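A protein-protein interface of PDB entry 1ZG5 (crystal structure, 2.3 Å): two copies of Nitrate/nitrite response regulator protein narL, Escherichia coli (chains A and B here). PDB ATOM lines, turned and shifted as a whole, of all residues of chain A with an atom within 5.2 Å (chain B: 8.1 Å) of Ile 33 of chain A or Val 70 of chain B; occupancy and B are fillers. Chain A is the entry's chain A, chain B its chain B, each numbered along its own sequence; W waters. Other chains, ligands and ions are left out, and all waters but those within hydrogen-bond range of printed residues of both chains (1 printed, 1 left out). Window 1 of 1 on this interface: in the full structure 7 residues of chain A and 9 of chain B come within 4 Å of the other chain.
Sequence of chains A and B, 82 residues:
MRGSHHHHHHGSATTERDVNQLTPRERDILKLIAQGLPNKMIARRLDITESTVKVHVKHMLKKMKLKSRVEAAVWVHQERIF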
ATOM      1  N   ILE A  29      15.354 -20.617   1.229  1.00  0.00           N
ATOM      2  CA  ILE A  29      15.068 -19.372   0.520  1.00  0.00           C
ATOM      3  C   ILE A  29      13.899 -19.539  -0.470  1.00  0.00           C
ATOM      4  O   ILE A  29      12.984 -18.732  -0.496  1.00  0.00           O
ATOM      5  CB  ILE A  29      16.349 -18.824  -0.245  1.00  0.00           C
ATOM      6  CG1 ILE A  29      17.307 -18.103   0.717  1.00  0.00           C
ATOM      7  CG2 ILE A  29      15.936 -17.825  -1.330  1.00  0.00           C
ATOM      8  CD1 ILE A  29      17.942 -18.989   1.742  1.00  0.00           C
ATOM      9  N   LEU A  30      13.928 -20.581  -1.283  1.00  0.00           N
ATOM     10  CA  LEU A  30      12.857 -20.775  -2.236  1.00  0.00           C
ATOM     11  C   LEU A  30      11.500 -20.794  -1.548  1.00  0.00           C
ATOM     12  O   LEU A  30      10.535 -20.284  -2.086  1.00  0.00           O
ATOM     13  CB  LEU A  30      13.069 -22.078  -3.004  1.00  0.00           C
ATOM     14  CG  LEU A  30      12.000 -22.350  -4.076  1.00  0.00           C
ATOM     15  CD1 LEU A  30      12.046 -21.281  -5.143  1.00  0.00           C
ATOM     16  CD2 LEU A  30      12.181 -23.737  -4.681  1.00  0.00           C
ATOM     17  N   LYS A  31      11.418 -21.415  -0.376  1.00  0.00           N
ATOM     18  CA  LYS A  31      10.160 -21.482   0.358  1.00  0.00           C
ATOM     19  C   LYS A  31       9.683 -20.092   0.769  1.00  0.00           C
ATOM     20  O   LYS A  31       8.516 -19.762   0.595  1.00  0.00           O
ATOM     21  CB  LYS A  31      10.322 -22.360   1.597  1.00  0.00           C
ATOM     22  CG  LYS A  31      10.511 -23.830   1.296  1.00  0.00           C
ATOM     23  CD  LYS A  31      10.693 -24.663   2.566  1.00  0.00           C
ATOM     24  CE  LYS A  31      10.984 -26.119   2.223  1.00  0.00           C
ATOM     25  NZ  LYS A  31      11.136 -26.986   3.408  1.00  0.00           N
ATOM     26  N   LEU A  32      10.574 -19.284   1.324  1.00  0.00           N
ATOM     27  CA  LEU A  32      10.201 -17.941   1.724  1.00  0.00           C
ATOM     28  C   LEU A  32       9.863 -17.090   0.508  1.00  0.00           C
ATOM     29  O   LEU A  32       8.959 -16.280   0.554  1.00  0.00           O
ATOM     30  CB  LEU A  32      11.322 -17.328   2.559  1.00  0.00           C
ATOM     31  CG  LEU A  32      11.205 -17.559   4.082  1.00  0.00           C
ATOM     32  CD1 LEU A  32      10.338 -18.785   4.389  1.00  0.00           C
ATOM     33  CD2 LEU A  32      12.603 -17.737   4.675  1.00  0.00           C
ATOM     34  N   ILE A  33      10.577 -17.286  -0.591  1.00  0.00           N
ATOM     35  CA  ILE A  33      10.274 -16.560  -1.826  1.00  0.00           C
ATOM     36  C   ILE A  33       8.850 -16.905  -2.285  1.00  0.00           C
ATOM     37  O   ILE A  33       8.071 -16.020  -2.631  1.00  0.00           O
ATOM     38  CB  ILE A  33      11.270 -16.927  -2.970  1.00  0.00           C
ATOM     39  CG1 ILE A  33      12.565 -16.125  -2.811  1.00  0.00           C
ATOM     40  CG2 ILE A  33      10.637 -16.675  -4.326  1.00  0.00           C
ATOM     41  CD1 ILE A  33      13.606 -16.426  -3.806  1.00  0.00           C
ATOM     42  N   ALA A  34       8.536 -18.197  -2.313  1.00  0.00           N
ATOM     43  CA  ALA A  34       7.229 -18.673  -2.719  1.00  0.00           C
ATOM     44  C   ALA A  34       6.133 -18.148  -1.793  1.00  0.00           C
ATOM     45  O   ALA A  34       4.955 -18.212  -2.134  1.00  0.00           O
ATOM     46  CB  ALA A  34       7.226 -20.184  -2.748  1.00  0.00           C
ATOM     47  N   GLN A  35       6.519 -17.619  -0.639  1.00  0.00           N
ATOM     48  CA  GLN A  35       5.542 -17.061   0.275  1.00  0.00           C
ATOM     49  C   GLN A  35       5.403 -15.572   0.035  1.00  0.00           C
ATOM     50  O   GLN A  35       4.639 -14.908   0.718  1.00  0.00           O
ATOM     51  CB  GLN A  35       5.960 -17.335   1.712  1.00  0.00           C
ATOM     52  CG  GLN A  35       5.432 -18.660   2.225  1.00  0.00           C
ATOM     53  CD  GLN A  35       6.143 -19.125   3.457  1.00  0.00           C
ATOM     54  OE1 GLN A  35       6.421 -18.332   4.353  1.00  0.00           O
ATOM     55  NE2 GLN A  35       6.439 -20.423   3.524  1.00  0.00           N
ATOM     56  N   GLY A  36       6.158 -15.066  -0.941  1.00  0.00           N
ATOM     57  CA  GLY A  36       6.104 -13.658  -1.321  1.00  0.00           C
ATOM     58  C   GLY A  36       7.056 -12.681  -0.643  1.00  0.00           C
ATOM     59  O   GLY A  36       6.898 -11.471  -0.820  1.00  0.00           O
ATOM     60  N   LEU A  37       8.043 -13.179   0.102  1.00  0.00           N
ATOM     61  CA  LEU A  37       8.986 -12.316   0.819  1.00  0.00           C
ATOM     62  C   LEU A  37      10.146 -11.720   0.031  1.00  0.00           C
ATOM     63  O   LEU A  37      10.758 -12.417  -0.798  1.00  0.00           O
ATOM     64  CB  LEU A  37       9.561 -13.063   2.016  1.00  0.00           C
ATOM     65  CG  LEU A  37       8.735 -13.108   3.291  1.00  0.00           C
ATOM     66  CD1 LEU A  37       7.352 -13.609   2.971  1.00  0.00           C
ATOM     67  CD2 LEU A  37       9.426 -13.998   4.306  1.00  0.00           C
ATOM     68  N   ASN A  39      13.968 -10.104  -0.397  1.00  0.00           N
ATOM     69  CA  ASN A  39      15.212 -10.597   0.185  1.00  0.00           C
ATOM     70  C   ASN A  39      15.498 -10.086   1.604  1.00  0.00           C
ATOM     71  O   ASN A  39      15.944 -10.867   2.443  1.00  0.00           O
ATOM     72  CB  ASN A  39      16.416 -10.294  -0.735  1.00  0.00           C
ATOM     73  CG  ASN A  39      16.341 -11.026  -2.067  1.00  0.00           C
ATOM     74  OD1 ASN A  39      15.781 -12.114  -2.173  1.00  0.00           O
ATOM     75  ND2 ASN A  39      16.928 -10.436  -3.082  1.00  0.00           N
ATOM     76  N   ILE A  42      13.530 -12.041   4.113  1.00  0.00           N
ATOM     77  CA  ILE A  42      14.046 -13.404   4.169  1.00  0.00           C
ATOM     78  C   ILE A  42      15.307 -13.422   5.036  1.00  0.00           C
ATOM     79  O   ILE A  42      15.542 -14.370   5.773  1.00  0.00           O
ATOM     80  CB  ILE A  42      14.424 -13.940   2.760  1.00  0.00           C
ATOM     81  CG1 ILE A  42      13.186 -14.001   1.860  1.00  0.00           C
ATOM     82  CG2 ILE A  42      15.071 -15.321   2.877  1.00  0.00           C
ATOM     83  CD1 ILE A  42      13.494 -14.460   0.440  1.00  0.00           C
ATOM     84  N   VAL A  57      19.847 -17.040  -3.600  1.00  0.00           N
ATOM     85  CA  VAL A  57      18.845 -16.789  -4.622  1.00  0.00           C
ATOM     86  C   VAL A  57      19.402 -16.995  -6.014  1.00  0.00           C
ATOM     87  O   VAL A  57      18.820 -17.729  -6.785  1.00  0.00           O
ATOM     88  CB  VAL A  57      18.273 -15.361  -4.534  1.00  0.00           C
ATOM     89  CG1 VAL A  57      17.336 -15.103  -5.676  1.00  0.00           C
ATOM     90  CG2 VAL A  57      17.547 -15.179  -3.223  1.00  0.00           C
ATOM     91  N   MET A  60      20.169 -20.701  -6.629  1.00  0.00           N
ATOM     92  CA  MET A  60      18.908 -21.405  -6.855  1.00  0.00           C
ATOM     93  C   MET A  60      18.358 -21.133  -8.278  1.00  0.00           C
ATOM     94  O   MET A  60      17.939 -22.049  -8.996  1.00  0.00           O
ATOM     95  CB  MET A  60      17.890 -20.971  -5.780  1.00  0.00           C
ATOM     96  CG  MET A  60      16.492 -21.611  -5.894  1.00  0.00           C
ATOM     97  SD  MET A  60      15.284 -20.756  -7.205  1.00  0.00           S
ATOM     98  CE  MET A  60      15.003 -19.091  -6.208  1.00  0.00           C
ATOM     99  N   ARG A  69      12.647 -14.415  -9.406  1.00  0.00           N
ATOM    100  CA  ARG A  69      12.051 -14.951  -8.188  1.00  0.00           C
ATOM    101  C   ARG A  69      10.548 -15.152  -8.384  1.00  0.00           C
ATOM    102  O   ARG A  69       9.952 -16.033  -7.763  1.00  0.00           O
ATOM    103  CB  ARG A  69      12.313 -14.010  -7.016  1.00  0.00           C
ATOM    104  CG  ARG A  69      11.639 -12.675  -7.157  1.00  0.00           C
ATOM    105  CD  ARG A  69      12.234 -11.620  -6.256  1.00  0.00           C
ATOM    106  NE  ARG A  69      12.131 -11.890  -4.822  1.00  0.00           N
ATOM    107  CZ  ARG A  69      13.145 -12.264  -4.047  1.00  0.00           C
ATOM    108  NH1 ARG A  69      14.351 -12.440  -4.553  1.00  0.00           N
ATOM    109  NH2 ARG A  69      12.982 -12.404  -2.744  1.00  0.00           N
ATOM    110  N   VAL A  70       9.920 -14.347  -9.243  1.00  0.00           N
ATOM    111  CA  VAL A  70       8.487 -14.544  -9.462  1.00  0.00           C
ATOM    112  C   VAL A  70       8.277 -15.883 -10.186  1.00  0.00           C
ATOM    113  O   VAL A  70       7.331 -16.607  -9.905  1.00  0.00           O
ATOM    114  CB  VAL A  70       7.841 -13.416 -10.309  1.00  0.00           C
ATOM    115  CG1 VAL A  70       6.354 -13.646 -10.432  1.00  0.00           C
ATOM    116  CG2 VAL A  70       8.090 -12.102  -9.672  1.00  0.00           C
ATOM    117  N   ALA A  72      10.134 -18.479  -9.911  1.00  0.00           N
ATOM    118  CA  ALA A  72      10.343 -19.489  -8.880  1.00  0.00           C
ATOM    119  C   ALA A  72       9.119 -19.617  -7.957  1.00  0.00           C
ATOM    120  O   ALA A  72       8.786 -20.720  -7.537  1.00  0.00           O
ATOM    121  CB  ALA A  72      11.560 -19.141  -8.068  1.00  0.00           C
ATOM    122  N   ALA A  73       8.464 -18.499  -7.648  1.00  0.00           N
ATOM    123  CA  ALA A  73       7.281 -18.492  -6.786  1.00  0.00           C
ATOM    124  C   ALA A  73       6.156 -19.235  -7.493  1.00  0.00           C
ATOM    125  O   ALA A  73       5.525 -20.121  -6.908  1.00  0.00           O
ATOM    126  CB  ALA A  73       6.858 -17.059  -6.497  1.00  0.00           C
ATOM    127  N   ILE B  33       1.156 -11.587 -14.607  1.00  0.00           N
ATOM    128  CA  ILE B  33       2.129 -11.563 -13.513  1.00  0.00           C
ATOM    129  C   ILE B  33       2.079 -12.897 -12.783  1.00  0.00           C
ATOM    130  O   ILE B  33       3.117 -13.465 -12.469  1.00  0.00           O
ATOM    131  CB  ILE B  33       1.836 -10.417 -12.498  1.00  0.00           C
ATOM    132  CG1 ILE B  33       2.340  -9.092 -13.050  1.00  0.00           C
ATOM    133  CG2 ILE B  33       2.459 -10.708 -11.175  1.00  0.00           C
ATOM    134  CD1 ILE B  33       2.122  -7.958 -12.153  1.00  0.00           C
ATOM    135  N   ALA B  34       0.872 -13.388 -12.504  1.00  0.00           N
ATOM    136  CA  ALA B  34       0.708 -14.672 -11.814  1.00  0.00           C
ATOM    137  C   ALA B  34       1.272 -15.828 -12.647  1.00  0.00           C
ATOM    138  O   ALA B  34       1.407 -16.950 -12.157  1.00  0.00           O
ATOM    139  CB  ALA B  34      -0.755 -14.925 -11.521  1.00  0.00           C
ATOM    140  N   MET B  60      -2.919  -1.604  -9.635  1.00  0.00           N
ATOM    141  CA  MET B  60      -3.359  -2.883  -9.089  1.00  0.00           C
ATOM    142  C   MET B  60      -2.794  -3.094  -7.675  1.00  0.00           C
ATOM    143  O   MET B  60      -3.545  -3.422  -6.759  1.00  0.00           O
ATOM    144  CB  MET B  60      -2.913  -4.015 -10.030  1.00  0.00           C
ATOM    145  CG  MET B  60      -3.310  -5.416  -9.616  1.00  0.00           C
ATOM    146  SD  MET B  60      -2.155  -6.387  -8.421  1.00  0.00           S
ATOM    147  CE  MET B  60      -0.597  -6.580  -9.593  1.00  0.00           C
ATOM    148  N   LEU B  61      -1.486  -2.888  -7.496  1.00  0.00           N
ATOM    149  CA  LEU B  61      -0.839  -3.100  -6.200  1.00  0.00           C
ATOM    150  C   LEU B  61      -1.417  -2.248  -5.081  1.00  0.00           C
ATOM    151  O   LEU B  61      -1.635  -2.746  -3.993  1.00  0.00           O
ATOM    152  CB  LEU B  61       0.675  -2.870  -6.302  1.00  0.00           C
ATOM    153  CG  LEU B  61       1.565  -3.859  -7.063  1.00  0.00           C
ATOM    154  CD1 LEU B  61       3.011  -3.387  -6.926  1.00  0.00           C
ATOM    155  CD2 LEU B  61       1.398  -5.264  -6.499  1.00  0.00           C
ATOM    156  N   LEU B  66      -1.054  -4.913  -1.999  1.00  0.00           N
ATOM    157  CA  LEU B  66       0.069  -5.841  -2.126  1.00  0.00           C
ATOM    158  C   LEU B  66       1.334  -4.991  -2.236  1.00  0.00           C
ATOM    159  O   LEU B  66       1.297  -3.893  -2.774  1.00  0.00           O
ATOM    160  CB  LEU B  66      -0.086  -6.732  -3.362  1.00  0.00           C
ATOM    161  CG  LEU B  66      -0.892  -8.037  -3.293  1.00  0.00           C
ATOM    162  CD1 LEU B  66      -1.493  -8.226  -1.922  1.00  0.00           C
ATOM    163  CD2 LEU B  66      -1.961  -8.021  -4.369  1.00  0.00           C
ATOM    164  N   LYS B  67       2.444  -5.495  -1.710  1.00  0.00           N
ATOM    165  CA  LYS B  67       3.688  -4.742  -1.718  1.00  0.00           C
ATOM    166  C   LYS B  67       4.577  -4.984  -2.928  1.00  0.00           C
ATOM    167  O   LYS B  67       5.473  -4.183  -3.198  1.00  0.00           O
ATOM    168  CB  LYS B  67       4.483  -5.051  -0.450  1.00  0.00           C
ATOM    169  CG  LYS B  67       3.685  -4.887   0.826  1.00  0.00           C
ATOM    170  CD  LYS B  67       4.419  -5.488   2.017  1.00  0.00           C
ATOM    171  CE  LYS B  67       3.561  -5.411   3.272  1.00  0.00           C
ATOM    172  NZ  LYS B  67       4.199  -6.072   4.442  1.00  0.00           N
ATOM    173  N   SER B  68       4.338  -6.076  -3.647  1.00  0.00           N
ATOM    174  CA  SER B  68       5.151  -6.392  -4.819  1.00  0.00           C
ATOM    175  C   SER B  68       4.433  -7.316  -5.775  1.00  0.00           C
ATOM    176  O   SER B  68       3.398  -7.893  -5.439  1.00  0.00           O
ATOM    177  CB  SER B  68       6.442  -7.064  -4.393  1.00  0.00           C
ATOM    178  OG  SER B  68       6.180  -8.377  -3.959  1.00  0.00           O
ATOM    179  N   ARG B  69       4.979  -7.443  -6.982  1.00  0.00           N
ATOM    180  CA  ARG B  69       4.384  -8.312  -7.986  1.00  0.00           C
ATOM    181  C   ARG B  69       4.453  -9.772  -7.525  1.00  0.00           C
ATOM    182  O   ARG B  69       3.648 -10.600  -7.954  1.00  0.00           O
ATOM    183  CB  ARG B  69       5.090  -8.148  -9.328  1.00  0.00           C
ATOM    184  CG  ARG B  69       6.457  -8.757  -9.396  1.00  0.00           C
ATOM    185  CD  ARG B  69       7.290  -8.192 -10.539  1.00  0.00           C
ATOM    186  NE  ARG B  69       6.809  -8.501 -11.882  1.00  0.00           N
ATOM    187  CZ  ARG B  69       6.157  -7.657 -12.668  1.00  0.00           C
ATOM    188  NH1 ARG B  69       5.881  -6.437 -12.265  1.00  0.00           N
ATOM    189  NH2 ARG B  69       5.793  -8.026 -13.877  1.00  0.00           N
ATOM    190  N   VAL B  70       5.400 -10.085  -6.647  1.00  0.00           N
ATOM    191  CA  VAL B  70       5.528 -11.444  -6.136  1.00  0.00           C
ATOM    192  C   VAL B  70       4.403 -11.781  -5.178  1.00  0.00           C
ATOM    193  O   VAL B  70       3.905 -12.888  -5.209  1.00  0.00           O
ATOM    194  CB  VAL B  70       6.842 -11.670  -5.384  1.00  0.00           C
ATOM    195  CG1 VAL B  70       6.998 -13.130  -5.063  1.00  0.00           C
ATOM    196  CG2 VAL B  70       7.993 -11.193  -6.219  1.00  0.00           C
ATOM    197  N   GLU B  71       4.028 -10.848  -4.306  1.00  0.00           N
ATOM    198  CA  GLU B  71       2.929 -11.087  -3.374  1.00  0.00           C
ATOM    199  C   GLU B  71       1.675 -11.242  -4.204  1.00  0.00           C
ATOM    200  O   GLU B  71       0.841 -12.070  -3.897  1.00  0.00           O
ATOM    201  CB  GLU B  71       2.736  -9.911  -2.420  1.00  0.00           C
ATOM    202  CG  GLU B  71       3.892  -9.637  -1.491  1.00  0.00           C
ATOM    203  CD  GLU B  71       3.470  -8.824  -0.294  1.00  0.00           C
ATOM    204  OE1 GLU B  71       2.503  -8.052  -0.419  1.00  0.00           O
ATOM    205  OE2 GLU B  71       4.108  -8.950   0.769  1.00  0.00           O
ATOM    206  N   ALA B  72       1.548 -10.433  -5.253  1.00  0.00           N
ATOM    207  CA  ALA B  72       0.394 -10.496  -6.149  1.00  0.00           C
ATOM    208  C   ALA B  72       0.294 -11.876  -6.815  1.00  0.00           C
ATOM    209  O   ALA B  72      -0.795 -12.432  -6.914  1.00  0.00           O
ATOM    210  CB  ALA B  72       0.496  -9.414  -7.209  1.00  0.00           C
ATOM    211  N   ALA B  73       1.421 -12.419  -7.267  1.00  0.00           N
ATOM    212  CA  ALA B  73       1.456 -13.733  -7.905  1.00  0.00           C
ATOM    213  C   ALA B  73       1.108 -14.828  -6.888  1.00  0.00           C
ATOM    214  O   ALA B  73       0.327 -15.728  -7.197  1.00  0.00           O
ATOM    215  CB  ALA B  73       2.836 -13.988  -8.488  1.00  0.00           C
ATOM    216  N   VAL B  74       1.694 -14.752  -5.691  1.00  0.00           N
ATOM    217  CA  VAL B  74       1.459 -15.737  -4.642  1.00  0.00           C
ATOM    218  C   VAL B  74       0.017 -15.690  -4.166  1.00  0.00           C
ATOM    219  O   VAL B  74      -0.572 -16.723  -3.894  1.00  0.00           O
ATOM    220  CB  VAL B  74       2.403 -15.505  -3.459  1.00  0.00           C
ATOM    221  CG1 VAL B  74       1.981 -16.342  -2.295  1.00  0.00           C
ATOM    222  CG2 VAL B  74       3.812 -15.843  -3.867  1.00  0.00           C
ATOM    223  N   TRP B  75      -0.549 -14.489  -4.072  1.00  0.00           N
ATOM    224  CA  TRP B  75      -1.941 -14.321  -3.662  1.00  0.00           C
ATOM    225  C   TRP B  75      -2.851 -15.008  -4.677  1.00  0.00           C
ATOM    226  O   TRP B  75      -3.699 -15.816  -4.304  1.00  0.00           O
ATOM    227  CB  TRP B  75      -2.296 -12.830  -3.582  1.00  0.00           C
ATOM    228  CG  TRP B  75      -3.765 -12.560  -3.483  1.00  0.00           C
ATOM    229  CD1 TRP B  75      -4.625 -13.049  -2.546  1.00  0.00           C
ATOM    230  CD2 TRP B  75      -4.549 -11.739  -4.356  1.00  0.00           C
ATOM    231  NE1 TRP B  75      -5.898 -12.584  -2.778  1.00  0.00           N
ATOM    232  CE2 TRP B  75      -5.880 -11.768  -3.883  1.00  0.00           C
ATOM    233  CE3 TRP B  75      -4.255 -10.968  -5.493  1.00  0.00           C
ATOM    234  CZ2 TRP B  75      -6.922 -11.067  -4.506  1.00  0.00           C
ATOM    235  CZ3 TRP B  75      -5.290 -10.268  -6.116  1.00  0.00           C
ATOM    236  CH2 TRP B  75      -6.606 -10.319  -5.617  1.00  0.00           C
ATOM    237  N   VAL B  76      -2.662 -14.685  -5.955  1.00  0.00           N
ATOM    238  CA  VAL B  76      -3.469 -15.262  -7.025  1.00  0.00           C
ATOM    239  C   VAL B  76      -3.501 -16.791  -6.980  1.00  0.00           C
ATOM    240  O   VAL B  76      -4.544 -17.399  -7.197  1.00  0.00           O
ATOM    241  CB  VAL B  76      -2.969 -14.788  -8.400  1.00  0.00           C
ATOM    242  CG1 VAL B  76      -3.479 -15.701  -9.479  1.00  0.00           C
ATOM    243  CG2 VAL B  76      -3.441 -13.381  -8.647  1.00  0.00           C
ATOM    244  N   HIS B  77      -2.366 -17.414  -6.681  1.00  0.00           N
ATOM    245  CA  HIS B  77      -2.308 -18.875  -6.610  1.00  0.00           C
ATOM    246  C   HIS B  77      -2.911 -19.464  -5.338  1.00  0.00           C
ATOM    247  O   HIS B  77      -3.669 -20.432  -5.411  1.00  0.00           O
ATOM    248  CB  HIS B  77      -0.869 -19.372  -6.779  1.00  0.00           C
ATOM    249  CG  HIS B  77      -0.396 -19.356  -8.202  1.00  0.00           C
ATOM    250  ND1 HIS B  77       0.138 -18.238  -8.801  1.00  0.00           N
ATOM    251  CD2 HIS B  77      -0.445 -20.311  -9.163  1.00  0.00           C
ATOM    252  CE1 HIS B  77       0.396 -18.501 -10.073  1.00  0.00           C
ATOM    253  NE2 HIS B  77       0.048 -19.751 -10.317  1.00  0.00           N
HETATM  254  O   HOH W   1       8.092  -9.186  -2.168  1.00  0.00           O
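Of the 16 printed residues of chain B, 5 touch a printed residue of chain A. Among the printed residues, 8 pairs touch across the chains. Among the printed residues, no Asp or Glu carboxylate lies within 4 Å of a Lys or Arg side-chain nitrogen of the other chain.
The side-chain carboxylate of Glu 71 of chain B sits at hydrogen-bond distance from the backbone NH of Lys 67 of chain B, 2.9 Å away. N of Glu 71 of chain B lies within hydrogen-bond range of OG of Ser 68 of chain B, at 3.3 Å. The side-chain hydroxyl (OG) of Ser 68 of chain B sits close to the backbone NH (N) of Val 70 of chain B (3.3 Å).
Ile 33 of chain A touches Val 70 of chain B, and with the chains exchanged Val 70 of chain A touches Ile 33 of chain B. Val 70 of chain A touches Arg 69 of chain B, but with the chains exchanged Arg 69 of chain A does not touch Val 70 of chain B (4.05 Å). Val 70 of chain B touches its own counterpart, Val 70 of chain A. Positions printed for both chains: 33, 34, 60, 69, 70, 72 and 73. Of the 8 pairs that touch across the chains among the printed residues, 3 have their exchanged pair printed and touching as well.
Water W1 bridges the side-chain hydroxyl (OG) of Ser 68 of chain B and the backbone carbonyl oxygen (O) of Gly 36 of chain A.
Ile 33 of chain A touches Val 70 of chain B. O of Ala 34 of chain A touches CG2 of Val 74 of chain B (3.1 Å). Gly 36 of chain A touches Val 70 of chain B. Gly 36 of chain A touches Glu 71 of chain B (O to CG, 3.6 Å). Gly 36 of chain A touches Val 74 of chain B. Val 70 of chain A touches Ile 33 of chain B (CG1 to O, 3.8 Å). CG2 of Val 70 of chain A touches CG of Arg 69 of chain B (3.7 Å). Val 70 of chain A touches Val 70 of chain B (CG2 to CG2, 3.6 Å).
Ile 33 of chain A touches just one residue of chain B: Val 70. Of the printed residues of chain B, Gly 36 of chain A touches Val 70 (3.9 Å), Glu 71 (3.6 Å) and Val 74 (3.8 Å). Of the printed residues of chain B, Val 70 of chain A touches Ile 33, Arg 69 and Val 70. Met 60 of chain B touches none of the printed residues of chain A. Lys 67 of chain B touches none of the printed residues of chain A. Of the printed residues of chain A, Arg 69 of chain B touches Val 70 (3.7 Å). Of the printed residues of chain A, Val 70 of chain B touches Ile 33 (3.9 Å), Gly 36 (3.9 Å) and Val 70 (3.6 Å). Of the printed residues of chain A, Val 74 of chain B touches Ala 34 and Gly 36. The nearest printed residue of chain B that does not touch Gly 36 of chain A is Ser 68 of chain B (4.5 Å).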
